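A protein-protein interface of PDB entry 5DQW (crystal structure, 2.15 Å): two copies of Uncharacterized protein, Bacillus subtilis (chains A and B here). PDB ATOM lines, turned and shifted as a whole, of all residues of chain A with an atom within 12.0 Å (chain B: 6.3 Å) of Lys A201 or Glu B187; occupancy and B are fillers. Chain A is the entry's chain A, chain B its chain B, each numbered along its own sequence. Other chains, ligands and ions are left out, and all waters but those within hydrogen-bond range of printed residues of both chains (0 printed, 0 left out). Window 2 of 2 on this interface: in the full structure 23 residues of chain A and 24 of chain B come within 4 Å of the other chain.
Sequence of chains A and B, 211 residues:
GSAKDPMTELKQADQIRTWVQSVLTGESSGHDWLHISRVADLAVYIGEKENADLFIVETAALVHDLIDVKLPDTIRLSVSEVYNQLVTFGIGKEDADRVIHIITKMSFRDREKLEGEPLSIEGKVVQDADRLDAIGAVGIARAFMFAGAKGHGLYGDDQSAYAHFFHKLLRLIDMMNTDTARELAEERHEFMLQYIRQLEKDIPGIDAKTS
The side-chain carboxylate (OD1) of Asp A202 lies within salt-bridge range of the guanidinium group (NE) of Arg B188.
SD of Met B192 sits close to N of Gly B136.
CZ of Phe B191 touches CZ of Phe A191, 3.9 Å away. CD2 of Tyr A195 touches CE2 of Phe B191, 3.7 Å away. Gln A198 touches Phe B191. Lys A201 touches Glu B187. C of Gly B136 touches OD2 of Asp A202, at 3.8 Å.
Leu A154 touches none of the printed residues of chain B. Printed residues of chain B within 4 Å of Phe A191: Phe B191. Of the printed residues of chain B, Tyr A195 touches Phe B191 (3.7 Å). Printed residues of chain B within 4 Å of Gln A198: Phe B191 (3.6 Å). Printed residues of chain B within 4 Å of Lys A201: Glu B187. Printed residues of chain B within 4 Å of Asp A202: Gly B136 and Arg B188. Gly B136 touches just one residue of chain A: Asp A202. Arg B182 touches none of the printed residues of chain A. No residue of chain A comes within 4 Å of Ala B185. Of chain A, only Lys A201 (3.8 Å) comes within 4 Å of Glu B187. Arg B188 touches just one residue of chain A: Asp A202 (3.5 Å). Of chain A, only Phe A191, Tyr A195 and Gln A198 come within 4 Å of Phe B191.
Of the 22 printed residues of chain A, 5 touch a printed residue of chain B. Along chain A the printed residues that touch a printed residue of chain B span positions 191 to 202. Among the printed residues, Asp or Glu carboxylates within 4 Å of a Lys or Arg side-chain nitrogen of the other chain: Asp A202 with Arg B188.
Phe B191 touches its own counterpart, Phe A191.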
ATOM      1  N   LEU A 154      27.685  21.031  -9.180  1.00  0.00           N
ATOM      2  CA  LEU A 154      27.266  20.326 -10.360  1.00  0.00           C
ATOM      3  C   LEU A 154      28.531  19.883 -11.098  1.00  0.00           C
ATOM      4  O   LEU A 154      28.656  18.736 -11.538  1.00  0.00           O
ATOM      5  CB  LEU A 154      26.431  21.275 -11.205  1.00  0.00           C
ATOM      6  CG  LEU A 154      25.425  20.708 -12.198  1.00  0.00           C
ATOM      7  CD1 LEU A 154      24.463  21.850 -12.578  1.00  0.00           C
ATOM      8  CD2 LEU A 154      26.104  20.062 -13.436  1.00  0.00           C
ATOM      9  N   TYR A 155      29.458  20.824 -11.217  1.00  0.00           N
ATOM     10  CA  TYR A 155      30.825  20.578 -11.714  1.00  0.00           C
ATOM     11  C   TYR A 155      31.754  21.535 -10.991  1.00  0.00           C
ATOM     12  O   TYR A 155      31.303  22.336 -10.190  1.00  0.00           O
ATOM     13  CB  TYR A 155      30.929  20.883 -13.201  1.00  0.00           C
ATOM     14  CG  TYR A 155      30.383  22.243 -13.578  1.00  0.00           C
ATOM     15  CD1 TYR A 155      29.034  22.402 -13.856  1.00  0.00           C
ATOM     16  CD2 TYR A 155      31.207  23.358 -13.690  1.00  0.00           C
ATOM     17  CE1 TYR A 155      28.523  23.619 -14.222  1.00  0.00           C
ATOM     18  CE2 TYR A 155      30.690  24.612 -14.051  1.00  0.00           C
ATOM     19  CZ  TYR A 155      29.336  24.716 -14.314  1.00  0.00           C
ATOM     20  OH  TYR A 155      28.738  25.899 -14.679  1.00  0.00           O
ATOM     21  N   TYR A 162      29.755  16.094 -11.589  1.00  0.00           N
ATOM     22  CA  TYR A 162      30.422  15.833 -12.893  1.00  0.00           C
ATOM     23  C   TYR A 162      31.707  15.014 -12.716  1.00  0.00           C
ATOM     24  O   TYR A 162      31.927  14.037 -13.452  1.00  0.00           O
ATOM     25  CB  TYR A 162      30.714  17.147 -13.606  1.00  0.00           C
ATOM     26  CG  TYR A 162      31.109  17.046 -15.064  1.00  0.00           C
ATOM     27  CD1 TYR A 162      30.213  16.607 -16.011  1.00  0.00           C
ATOM     28  CD2 TYR A 162      32.368  17.474 -15.497  1.00  0.00           C
ATOM     29  CE1 TYR A 162      30.564  16.539 -17.371  1.00  0.00           C
ATOM     30  CE2 TYR A 162      32.735  17.424 -16.842  1.00  0.00           C
ATOM     31  CZ  TYR A 162      31.823  16.944 -17.779  1.00  0.00           C
ATOM     32  OH  TYR A 162      32.150  16.867 -19.106  1.00  0.00           O
ATOM     33  N   PHE A 166      33.217  10.828 -14.048  1.00  0.00           N
ATOM     34  CA  PHE A 166      34.525  10.402 -14.538  1.00  0.00           C
ATOM     35  C   PHE A 166      35.266   9.469 -13.611  1.00  0.00           C
ATOM     36  O   PHE A 166      35.909   8.536 -14.072  1.00  0.00           O
ATOM     37  CB  PHE A 166      35.414  11.615 -14.950  1.00  0.00           C
ATOM     38  CG  PHE A 166      34.908  12.277 -16.185  1.00  0.00           C
ATOM     39  CD1 PHE A 166      33.838  13.144 -16.114  1.00  0.00           C
ATOM     40  CD2 PHE A 166      35.407  11.932 -17.425  1.00  0.00           C
ATOM     41  CE1 PHE A 166      33.291  13.706 -17.274  1.00  0.00           C
ATOM     42  CE2 PHE A 166      34.880  12.496 -18.568  1.00  0.00           C
ATOM     43  CZ  PHE A 166      33.826  13.392 -18.492  1.00  0.00           C
ATOM     44  N   PHE A 191      23.922   6.101 -23.036  1.00  0.00           N
ATOM     45  CA  PHE A 191      23.060   7.232 -22.743  1.00  0.00           C
ATOM     46  C   PHE A 191      23.748   8.218 -21.824  1.00  0.00           C
ATOM     47  O   PHE A 191      23.588   9.411 -21.997  1.00  0.00           O
ATOM     48  CB  PHE A 191      21.652   6.857 -22.229  1.00  0.00           C
ATOM     49  CG  PHE A 191      20.804   8.077 -22.008  1.00  0.00           C
ATOM     50  CD1 PHE A 191      20.171   8.687 -23.080  1.00  0.00           C
ATOM     51  CD2 PHE A 191      20.776   8.683 -20.770  1.00  0.00           C
ATOM     52  CE1 PHE A 191      19.460   9.853 -22.897  1.00  0.00           C
ATOM     53  CE2 PHE A 191      20.065   9.860 -20.571  1.00  0.00           C
ATOM     54  CZ  PHE A 191      19.416  10.449 -21.617  1.00  0.00           C
ATOM     55  N   MET A 192      24.536   7.754 -20.854  1.00  0.00           N
ATOM     56  CA  MET A 192      25.336   8.697 -20.000  1.00  0.00           C
ATOM     57  C   MET A 192      26.339   9.456 -20.831  1.00  0.00           C
ATOM     58  O   MET A 192      26.604  10.603 -20.566  1.00  0.00           O
ATOM     59  CB  MET A 192      26.113   8.015 -18.867  1.00  0.00           C
ATOM     60  CG  MET A 192      25.275   7.547 -17.710  1.00  0.00           C
ATOM     61  SD  MET A 192      26.277   6.960 -16.341  1.00  0.00           S
ATOM     62  CE  MET A 192      27.423   5.795 -17.146  1.00  0.00           C
ATOM     63  N   LEU A 193      26.914   8.798 -21.828  1.00  0.00           N
ATOM     64  CA  LEU A 193      27.812   9.479 -22.750  1.00  0.00           C
ATOM     65  C   LEU A 193      27.099  10.614 -23.534  1.00  0.00           C
ATOM     66  O   LEU A 193      27.661  11.716 -23.675  1.00  0.00           O
ATOM     67  CB  LEU A 193      28.450   8.476 -23.700  1.00  0.00           C
ATOM     68  CG  LEU A 193      29.605   7.653 -23.100  1.00  0.00           C
ATOM     69  CD1 LEU A 193      30.184   6.670 -24.141  1.00  0.00           C
ATOM     70  CD2 LEU A 193      30.699   8.606 -22.535  1.00  0.00           C
ATOM     71  N   GLN A 194      25.896  10.325 -24.065  1.00  0.00           N
ATOM     72  CA  GLN A 194      25.058  11.339 -24.713  1.00  0.00           C
ATOM     73  C   GLN A 194      24.729  12.481 -23.715  1.00  0.00           C
ATOM     74  O   GLN A 194      24.685  13.639 -24.089  1.00  0.00           O
ATOM     75  CB  GLN A 194      23.781  10.724 -25.292  1.00  0.00           C
ATOM     76  CG  GLN A 194      24.026   9.723 -26.464  1.00  0.00           C
ATOM     77  CD  GLN A 194      22.743   9.028 -26.989  1.00  0.00           C
ATOM     78  OE1 GLN A 194      21.831   8.666 -26.228  1.00  0.00           O
ATOM     79  NE2 GLN A 194      22.707   8.795 -28.293  1.00  0.00           N
ATOM     80  N   TYR A 195      24.509  12.140 -22.449  1.00  0.00           N
ATOM     81  CA  TYR A 195      24.208  13.161 -21.405  1.00  0.00           C
ATOM     82  C   TYR A 195      25.411  14.084 -21.182  1.00  0.00           C
ATOM     83  O   TYR A 195      25.281  15.320 -21.165  1.00  0.00           O
ATOM     84  CB  TYR A 195      23.715  12.508 -20.088  1.00  0.00           C
ATOM     85  CG  TYR A 195      23.409  13.561 -19.078  1.00  0.00           C
ATOM     86  CD1 TYR A 195      24.406  14.029 -18.251  1.00  0.00           C
ATOM     87  CD2 TYR A 195      22.148  14.144 -18.979  1.00  0.00           C
ATOM     88  CE1 TYR A 195      24.180  15.018 -17.347  1.00  0.00           C
ATOM     89  CE2 TYR A 195      21.924  15.161 -18.044  1.00  0.00           C
ATOM     90  CZ  TYR A 195      22.958  15.581 -17.249  1.00  0.00           C
ATOM     91  OH  TYR A 195      22.828  16.588 -16.342  1.00  0.00           O
ATOM     92  N   ILE A 196      26.596  13.498 -21.076  1.00  0.00           N
ATOM     93  CA  ILE A 196      27.827  14.274 -20.900  1.00  0.00           C
ATOM     94  C   ILE A 196      28.072  15.161 -22.125  1.00  0.00           C
ATOM     95  O   ILE A 196      28.407  16.330 -22.018  1.00  0.00           O
ATOM     96  CB  ILE A 196      29.011  13.344 -20.601  1.00  0.00           C
ATOM     97  CG1 ILE A 196      28.819  12.764 -19.195  1.00  0.00           C
ATOM     98  CG2 ILE A 196      30.356  14.095 -20.732  1.00  0.00           C
ATOM     99  CD1 ILE A 196      29.476  11.479 -18.968  1.00  0.00           C
ATOM    100  N   ARG A 197      27.805  14.617 -23.296  1.00  0.00           N
ATOM    101  CA  ARG A 197      27.957  15.383 -24.515  1.00  0.00           C
ATOM    102  C   ARG A 197      27.050  16.636 -24.522  1.00  0.00           C
ATOM    103  O   ARG A 197      27.475  17.751 -24.873  1.00  0.00           O
ATOM    104  CB  ARG A 197      27.632  14.474 -25.670  1.00  0.00           C
ATOM    105  CG  ARG A 197      27.660  15.119 -26.956  1.00  0.00           C
ATOM    106  CD  ARG A 197      27.157  14.197 -28.056  1.00  0.00           C
ATOM    107  NE  ARG A 197      27.007  15.019 -29.247  1.00  0.00           N
ATOM    108  CZ  ARG A 197      26.505  14.601 -30.393  1.00  0.00           C
ATOM    109  NH1 ARG A 197      26.099  13.339 -30.515  1.00  0.00           N
ATOM    110  NH2 ARG A 197      26.437  15.441 -31.423  1.00  0.00           N
ATOM    111  N   GLN A 198      25.807  16.441 -24.110  1.00  0.00           N
ATOM    112  CA  GLN A 198      24.868  17.538 -24.016  1.00  0.00           C
ATOM    113  C   GLN A 198      25.293  18.546 -22.930  1.00  0.00           C
ATOM    114  O   GLN A 198      25.122  19.738 -23.106  1.00  0.00           O
ATOM    115  CB  GLN A 198      23.460  16.985 -23.772  1.00  0.00           C
ATOM    116  CG  GLN A 198      22.351  17.990 -24.004  1.00  0.00           C
ATOM    117  CD  GLN A 198      22.130  18.302 -25.460  1.00  0.00           C
ATOM    118  OE1 GLN A 198      22.273  17.442 -26.319  1.00  0.00           O
ATOM    119  NE2 GLN A 198      21.803  19.538 -25.744  1.00  0.00           N
ATOM    120  N   LEU A 199      25.859  18.095 -21.819  1.00  0.00           N
ATOM    121  CA  LEU A 199      26.346  19.028 -20.825  1.00  0.00           C
ATOM    122  C   LEU A 199      27.522  19.811 -21.385  1.00  0.00           C
ATOM    123  O   LEU A 199      27.636  20.995 -21.143  1.00  0.00           O
ATOM    124  CB  LEU A 199      26.839  18.342 -19.555  1.00  0.00           C
ATOM    125  CG  LEU A 199      25.954  18.150 -18.338  1.00  0.00           C
ATOM    126  CD1 LEU A 199      26.908  17.745 -17.193  1.00  0.00           C
ATOM    127  CD2 LEU A 199      25.088  19.401 -17.990  1.00  0.00           C
ATOM    128  N   GLU A 200      28.406  19.128 -22.121  1.00  0.00           N
ATOM    129  CA  GLU A 200      29.540  19.826 -22.737  1.00  0.00           C
ATOM    130  C   GLU A 200      29.061  20.924 -23.685  1.00  0.00           C
ATOM    131  O   GLU A 200      29.683  21.960 -23.726  1.00  0.00           O
ATOM    132  CB  GLU A 200      30.524  18.859 -23.390  1.00  0.00           C
ATOM    133  CG  GLU A 200      31.305  18.073 -22.353  1.00  0.00           C
ATOM    134  CD  GLU A 200      32.138  16.904 -22.943  1.00  0.00           C
ATOM    135  OE1 GLU A 200      31.710  16.274 -23.931  1.00  0.00           O
ATOM    136  OE2 GLU A 200      33.223  16.628 -22.393  1.00  0.00           O
ATOM    137  N   LYS A 201      27.921  20.724 -24.372  1.00  0.00           N
ATOM    138  CA  LYS A 201      27.319  21.793 -25.208  1.00  0.00           C
ATOM    139  C   LYS A 201      26.591  22.853 -24.405  1.00  0.00           C
ATOM    140  O   LYS A 201      26.705  24.012 -24.699  1.00  0.00           O
ATOM    141  CB  LYS A 201      26.285  21.256 -26.202  1.00  0.00           C
ATOM    142  CG  LYS A 201      26.809  20.387 -27.298  1.00  0.00           C
ATOM    143  CD  LYS A 201      25.722  20.171 -28.358  1.00  0.00           C
ATOM    144  CE  LYS A 201      25.594  18.710 -28.756  1.00  0.00           C
ATOM    145  N   ASP A 202      25.761  22.454 -23.452  1.00  0.00           N
ATOM    146  CA  ASP A 202      25.046  23.423 -22.646  1.00  0.00           C
ATOM    147  C   ASP A 202      26.043  24.305 -21.898  1.00  0.00           C
ATOM    148  O   ASP A 202      25.733  25.452 -21.620  1.00  0.00           O
ATOM    149  CB  ASP A 202      24.144  22.748 -21.592  1.00  0.00           C
ATOM    150  CG  ASP A 202      22.969  21.965 -22.184  1.00  0.00           C
ATOM    151  OD1 ASP A 202      22.689  22.058 -23.378  1.00  0.00           O
ATOM    152  OD2 ASP A 202      22.293  21.246 -21.406  1.00  0.00           O
ATOM    153  N   ILE A 203      27.203  23.760 -21.531  1.00  0.00           N
ATOM    154  CA  ILE A 203      28.179  24.470 -20.647  1.00  0.00           C
ATOM    155  C   ILE A 203      29.600  24.441 -21.217  1.00  0.00           C
ATOM    156  O   ILE A 203      30.414  23.612 -20.843  1.00  0.00           O
ATOM    157  CB  ILE A 203      28.240  23.843 -19.214  1.00  0.00           C
ATOM    158  CG1 ILE A 203      26.846  23.739 -18.588  1.00  0.00           C
ATOM    159  CG2 ILE A 203      29.198  24.626 -18.325  1.00  0.00           C
ATOM    160  CD1 ILE A 203      26.799  22.832 -17.368  1.00  0.00           C
ATOM    161  N   PRO A 204      29.914  25.370 -22.120  1.00  0.00           N
ATOM    162  CA  PRO A 204      31.259  25.375 -22.695  1.00  0.00           C
ATOM    163  C   PRO A 204      32.323  25.553 -21.599  1.00  0.00           C
ATOM    164  O   PRO A 204      32.108  26.299 -20.650  1.00  0.00           O
ATOM    165  CB  PRO A 204      31.232  26.575 -23.649  1.00  0.00           C
ATOM    166  CG  PRO A 204      29.791  26.745 -24.001  1.00  0.00           C
ATOM    167  CD  PRO A 204      29.021  26.355 -22.754  1.00  0.00           C
ATOM    168  N   GLY A 205      33.419  24.814 -21.702  1.00  0.00           N
ATOM    169  CA  GLY A 205      34.466  24.844 -20.686  1.00  0.00           C
ATOM    170  C   GLY A 205      34.177  24.092 -19.395  1.00  0.00           C
ATOM    171  O   GLY A 205      34.932  24.205 -18.437  1.00  0.00           O
ATOM    172  N   ILE A 206      33.102  23.305 -19.356  1.00  0.00           N
ATOM    173  CA  ILE A 206      32.750  22.580 -18.146  1.00  0.00           C
ATOM    174  C   ILE A 206      33.908  21.721 -17.613  1.00  0.00           C
ATOM    175  O   ILE A 206      34.082  21.593 -16.399  1.00  0.00           O
ATOM    176  CB  ILE A 206      31.495  21.689 -18.359  1.00  0.00           C
ATOM    177  CG1 ILE A 206      31.007  21.117 -17.023  1.00  0.00           C
ATOM    178  CG2 ILE A 206      31.768  20.552 -19.367  1.00  0.00           C
ATOM    179  CD1 ILE A 206      29.650  20.331 -17.142  1.00  0.00           C
ATOM    180  N   ASP A 207      34.681  21.129 -18.525  1.00  0.00           N
ATOM    181  CA  ASP A 207      35.777  20.243 -18.156  1.00  0.00           C
ATOM    182  C   ASP A 207      36.941  20.959 -17.448  1.00  0.00           C
ATOM    183  O   ASP A 207      37.592  20.355 -16.595  1.00  0.00           O
ATOM    184  CB  ASP A 207      36.283  19.480 -19.399  1.00  0.00           C
ATOM    185  CG  ASP A 207      35.282  18.452 -19.884  1.00  0.00           C
ATOM    186  OD1 ASP A 207      35.123  17.442 -19.172  1.00  0.00           O
ATOM    187  OD2 ASP A 207      34.631  18.648 -20.939  1.00  0.00           O
ATOM    188  N   ALA A 208      37.198  22.220 -17.798  1.00  0.00           N
ATOM    189  CA  ALA A 208      38.401  22.946 -17.304  1.00  0.00           C
ATOM    190  C   ALA A 208      38.197  23.437 -15.881  1.00  0.00           C
ATOM    191  O   ALA A 208      37.345  24.294 -15.663  1.00  0.00           O
ATOM    192  CB  ALA A 208      38.720  24.138 -18.203  1.00  0.00           C
ATOM    193  N   GLY B 136      17.243  21.372 -20.697  1.00  0.00           N
ATOM    194  CA  GLY B 136      18.350  20.578 -21.246  1.00  0.00           C
ATOM    195  C   GLY B 136      19.033  19.673 -20.232  1.00  0.00           C
ATOM    196  O   GLY B 136      18.475  19.362 -19.195  1.00  0.00           O
ATOM    197  N   ILE B 173      10.025  26.160 -22.927  1.00  0.00           N
ATOM    198  CA  ILE B 173      10.357  26.512 -24.310  1.00  0.00           C
ATOM    199  C   ILE B 173       9.321  27.498 -24.893  1.00  0.00           C
ATOM    200  O   ILE B 173       9.678  28.452 -25.601  1.00  0.00           O
ATOM    201  CB  ILE B 173      10.534  25.245 -25.209  1.00  0.00           C
ATOM    202  CG1 ILE B 173      10.920  25.643 -26.643  1.00  0.00           C
ATOM    203  CG2 ILE B 173       9.265  24.374 -25.189  1.00  0.00           C
ATOM    204  CD1 ILE B 173      11.591  24.536 -27.437  1.00  0.00           C
ATOM    205  N   ARG B 182      14.593  31.030 -28.256  1.00  0.00           N
ATOM    206  CA  ARG B 182      13.688  29.998 -28.792  1.00  0.00           C
ATOM    207  C   ARG B 182      14.455  28.907 -29.568  1.00  0.00           C
ATOM    208  O   ARG B 182      14.108  27.724 -29.493  1.00  0.00           O
ATOM    209  CB  ARG B 182      12.588  30.623 -29.673  1.00  0.00           C
ATOM    210  N   GLU B 183      15.502  29.308 -30.291  1.00  0.00           N
ATOM    211  CA  GLU B 183      16.288  28.373 -31.114  1.00  0.00           C
ATOM    212  C   GLU B 183      17.174  27.503 -30.241  1.00  0.00           C
ATOM    213  O   GLU B 183      17.215  26.274 -30.402  1.00  0.00           O
ATOM    214  CB  GLU B 183      17.141  29.132 -32.137  1.00  0.00           C
ATOM    215  CG  GLU B 183      16.335  29.900 -33.161  1.00  0.00           C
ATOM    216  CD  GLU B 183      17.116  31.055 -33.776  1.00  0.00           C
ATOM    217  OE1 GLU B 183      18.365  31.071 -33.654  1.00  0.00           O
ATOM    218  OE2 GLU B 183      16.482  31.946 -34.383  1.00  0.00           O
ATOM    219  N   LEU B 184      17.891  28.146 -29.320  1.00  0.00           N
ATOM    220  CA  LEU B 184      18.670  27.432 -28.293  1.00  0.00           C
ATOM    221  C   LEU B 184      17.810  26.440 -27.507  1.00  0.00           C
ATOM    222  O   LEU B 184      18.238  25.315 -27.239  1.00  0.00           O
ATOM    223  CB  LEU B 184      19.302  28.423 -27.305  1.00  0.00           C
ATOM    224  CG  LEU B 184      20.337  29.384 -27.861  1.00  0.00           C
ATOM    225  CD1 LEU B 184      20.660  30.471 -26.855  1.00  0.00           C
ATOM    226  CD2 LEU B 184      21.589  28.597 -28.250  1.00  0.00           C
ATOM    227  N   ALA B 185      16.597  26.861 -27.150  1.00  0.00           N
ATOM    228  CA  ALA B 185      15.695  26.032 -26.352  1.00  0.00           C
ATOM    229  C   ALA B 185      15.321  24.721 -27.053  1.00  0.00           C
ATOM    230  O   ALA B 185      15.118  23.703 -26.386  1.00  0.00           O
ATOM    231  CB  ALA B 185      14.430  26.806 -25.976  1.00  0.00           C
ATOM    232  N   GLU B 186      15.260  24.726 -28.379  1.00  0.00           N
ATOM    233  CA  GLU B 186      14.794  23.542 -29.111  1.00  0.00           C
ATOM    234  C   GLU B 186      15.605  22.269 -28.821  1.00  0.00           C
ATOM    235  O   GLU B 186      15.048  21.253 -28.414  1.00  0.00           O
ATOM    236  CB  GLU B 186      14.757  23.810 -30.617  1.00  0.00           C
ATOM    237  CG  GLU B 186      14.077  22.695 -31.404  1.00  0.00           C
ATOM    238  CD  GLU B 186      12.621  22.469 -30.987  1.00  0.00           C
ATOM    239  OE1 GLU B 186      11.729  23.113 -31.575  1.00  0.00           O
ATOM    240  OE2 GLU B 186      12.375  21.643 -30.075  1.00  0.00           O
ATOM    241  N   GLU B 187      16.916  22.325 -29.012  1.00  0.00           N
ATOM    242  CA  GLU B 187      17.772  21.159 -28.743  1.00  0.00           C
ATOM    243  C   GLU B 187      17.770  20.764 -27.246  1.00  0.00           C
ATOM    244  O   GLU B 187      17.728  19.583 -26.908  1.00  0.00           O
ATOM    245  CB  GLU B 187      19.198  21.419 -29.231  1.00  0.00           C
ATOM    246  CG  GLU B 187      19.966  20.143 -29.575  1.00  0.00           C
ATOM    247  CD  GLU B 187      21.244  20.408 -30.377  1.00  0.00           C
ATOM    248  OE1 GLU B 187      21.305  21.421 -31.123  1.00  0.00           O
ATOM    249  OE2 GLU B 187      22.184  19.591 -30.258  1.00  0.00           O
ATOM    250  N   ARG B 188      17.782  21.757 -26.356  1.00  0.00           N
ATOM    251  CA  ARG B 188      17.718  21.491 -24.931  1.00  0.00           C
ATOM    252  C   ARG B 188      16.426  20.772 -24.579  1.00  0.00           C
ATOM    253  O   ARG B 188      16.439  19.774 -23.866  1.00  0.00           O
ATOM    254  CB  ARG B 188      17.852  22.785 -24.126  1.00  0.00           C
ATOM    255  CG  ARG B 188      19.258  23.433 -24.245  1.00  0.00           C
ATOM    256  CD  ARG B 188      19.407  24.516 -23.175  1.00  0.00           C
ATOM    257  NE  ARG B 188      20.643  25.254 -23.336  1.00  0.00           N
ATOM    258  CZ  ARG B 188      21.398  25.740 -22.357  1.00  0.00           C
ATOM    259  NH1 ARG B 188      21.073  25.600 -21.069  1.00  0.00           N
ATOM    260  NH2 ARG B 188      22.508  26.381 -22.684  1.00  0.00           N
ATOM    261  N   HIS B 189      15.311  21.272 -25.093  1.00  0.00           N
ATOM    262  CA  HIS B 189      14.009  20.652 -24.891  1.00  0.00           C
ATOM    263  C   HIS B 189      13.926  19.219 -25.488  1.00  0.00           C
ATOM    264  O   HIS B 189      13.473  18.266 -24.820  1.00  0.00           O
ATOM    265  CB  HIS B 189      12.924  21.566 -25.480  1.00  0.00           C
ATOM    266  CG  HIS B 189      11.535  21.045 -25.296  1.00  0.00           C
ATOM    267  ND1 HIS B 189      10.828  21.202 -24.122  1.00  0.00           N
ATOM    268  CD2 HIS B 189      10.742  20.327 -26.123  1.00  0.00           C
ATOM    269  CE1 HIS B 189       9.649  20.620 -24.245  1.00  0.00           C
ATOM    270  NE2 HIS B 189       9.568  20.087 -25.450  1.00  0.00           N
ATOM    271  N   GLU B 190      14.335  19.065 -26.742  1.00  0.00           N
ATOM    272  CA  GLU B 190      14.375  17.741 -27.374  1.00  0.00           C
ATOM    273  C   GLU B 190      15.195  16.767 -26.511  1.00  0.00           C
ATOM    274  O   GLU B 190      14.728  15.664 -26.177  1.00  0.00           O
ATOM    275  CB  GLU B 190      14.953  17.870 -28.781  1.00  0.00           C
ATOM    276  CG  GLU B 190      14.861  16.633 -29.634  1.00  0.00           C
ATOM    277  CD  GLU B 190      13.458  16.048 -29.711  1.00  0.00           C
ATOM    278  OE1 GLU B 190      12.472  16.776 -29.985  1.00  0.00           O
ATOM    279  OE2 GLU B 190      13.356  14.835 -29.475  1.00  0.00           O
ATOM    280  N   PHE B 191      16.367  17.210 -26.041  1.00  0.00           N
ATOM    281  CA  PHE B 191      17.163  16.362 -25.160  1.00  0.00           C
ATOM    282  C   PHE B 191      16.428  15.970 -23.857  1.00  0.00           C
ATOM    283  O   PHE B 191      16.446  14.804 -23.459  1.00  0.00           O
ATOM    284  CB  PHE B 191      18.572  16.908 -24.862  1.00  0.00           C
ATOM    285  CG  PHE B 191      19.373  15.951 -24.030  1.00  0.00           C
ATOM    286  CD1 PHE B 191      19.864  14.788 -24.601  1.00  0.00           C
ATOM    287  CD2 PHE B 191      19.508  16.135 -22.659  1.00  0.00           C
ATOM    288  CE1 PHE B 191      20.534  13.850 -23.849  1.00  0.00           C
ATOM    289  CE2 PHE B 191      20.188  15.200 -21.878  1.00  0.00           C
ATOM    290  CZ  PHE B 191      20.711  14.049 -22.489  1.00  0.00           C
ATOM    291  N   MET B 192      15.751  16.905 -23.207  1.00  0.00           N
ATOM    292  CA  MET B 192      14.958  16.528 -22.036  1.00  0.00           C
ATOM    293  C   MET B 192      13.970  15.426 -22.351  1.00  0.00           C
ATOM    294  O   MET B 192      13.743  14.547 -21.525  1.00  0.00           O
ATOM    295  CB  MET B 192      14.185  17.699 -21.481  1.00  0.00           C
ATOM    296  CG  MET B 192      15.049  18.676 -20.709  1.00  0.00           C
ATOM    297  SD  MET B 192      14.035  19.802 -19.717  1.00  0.00           S
ATOM    298  CE  MET B 192      12.919  20.506 -20.965  1.00  0.00           C
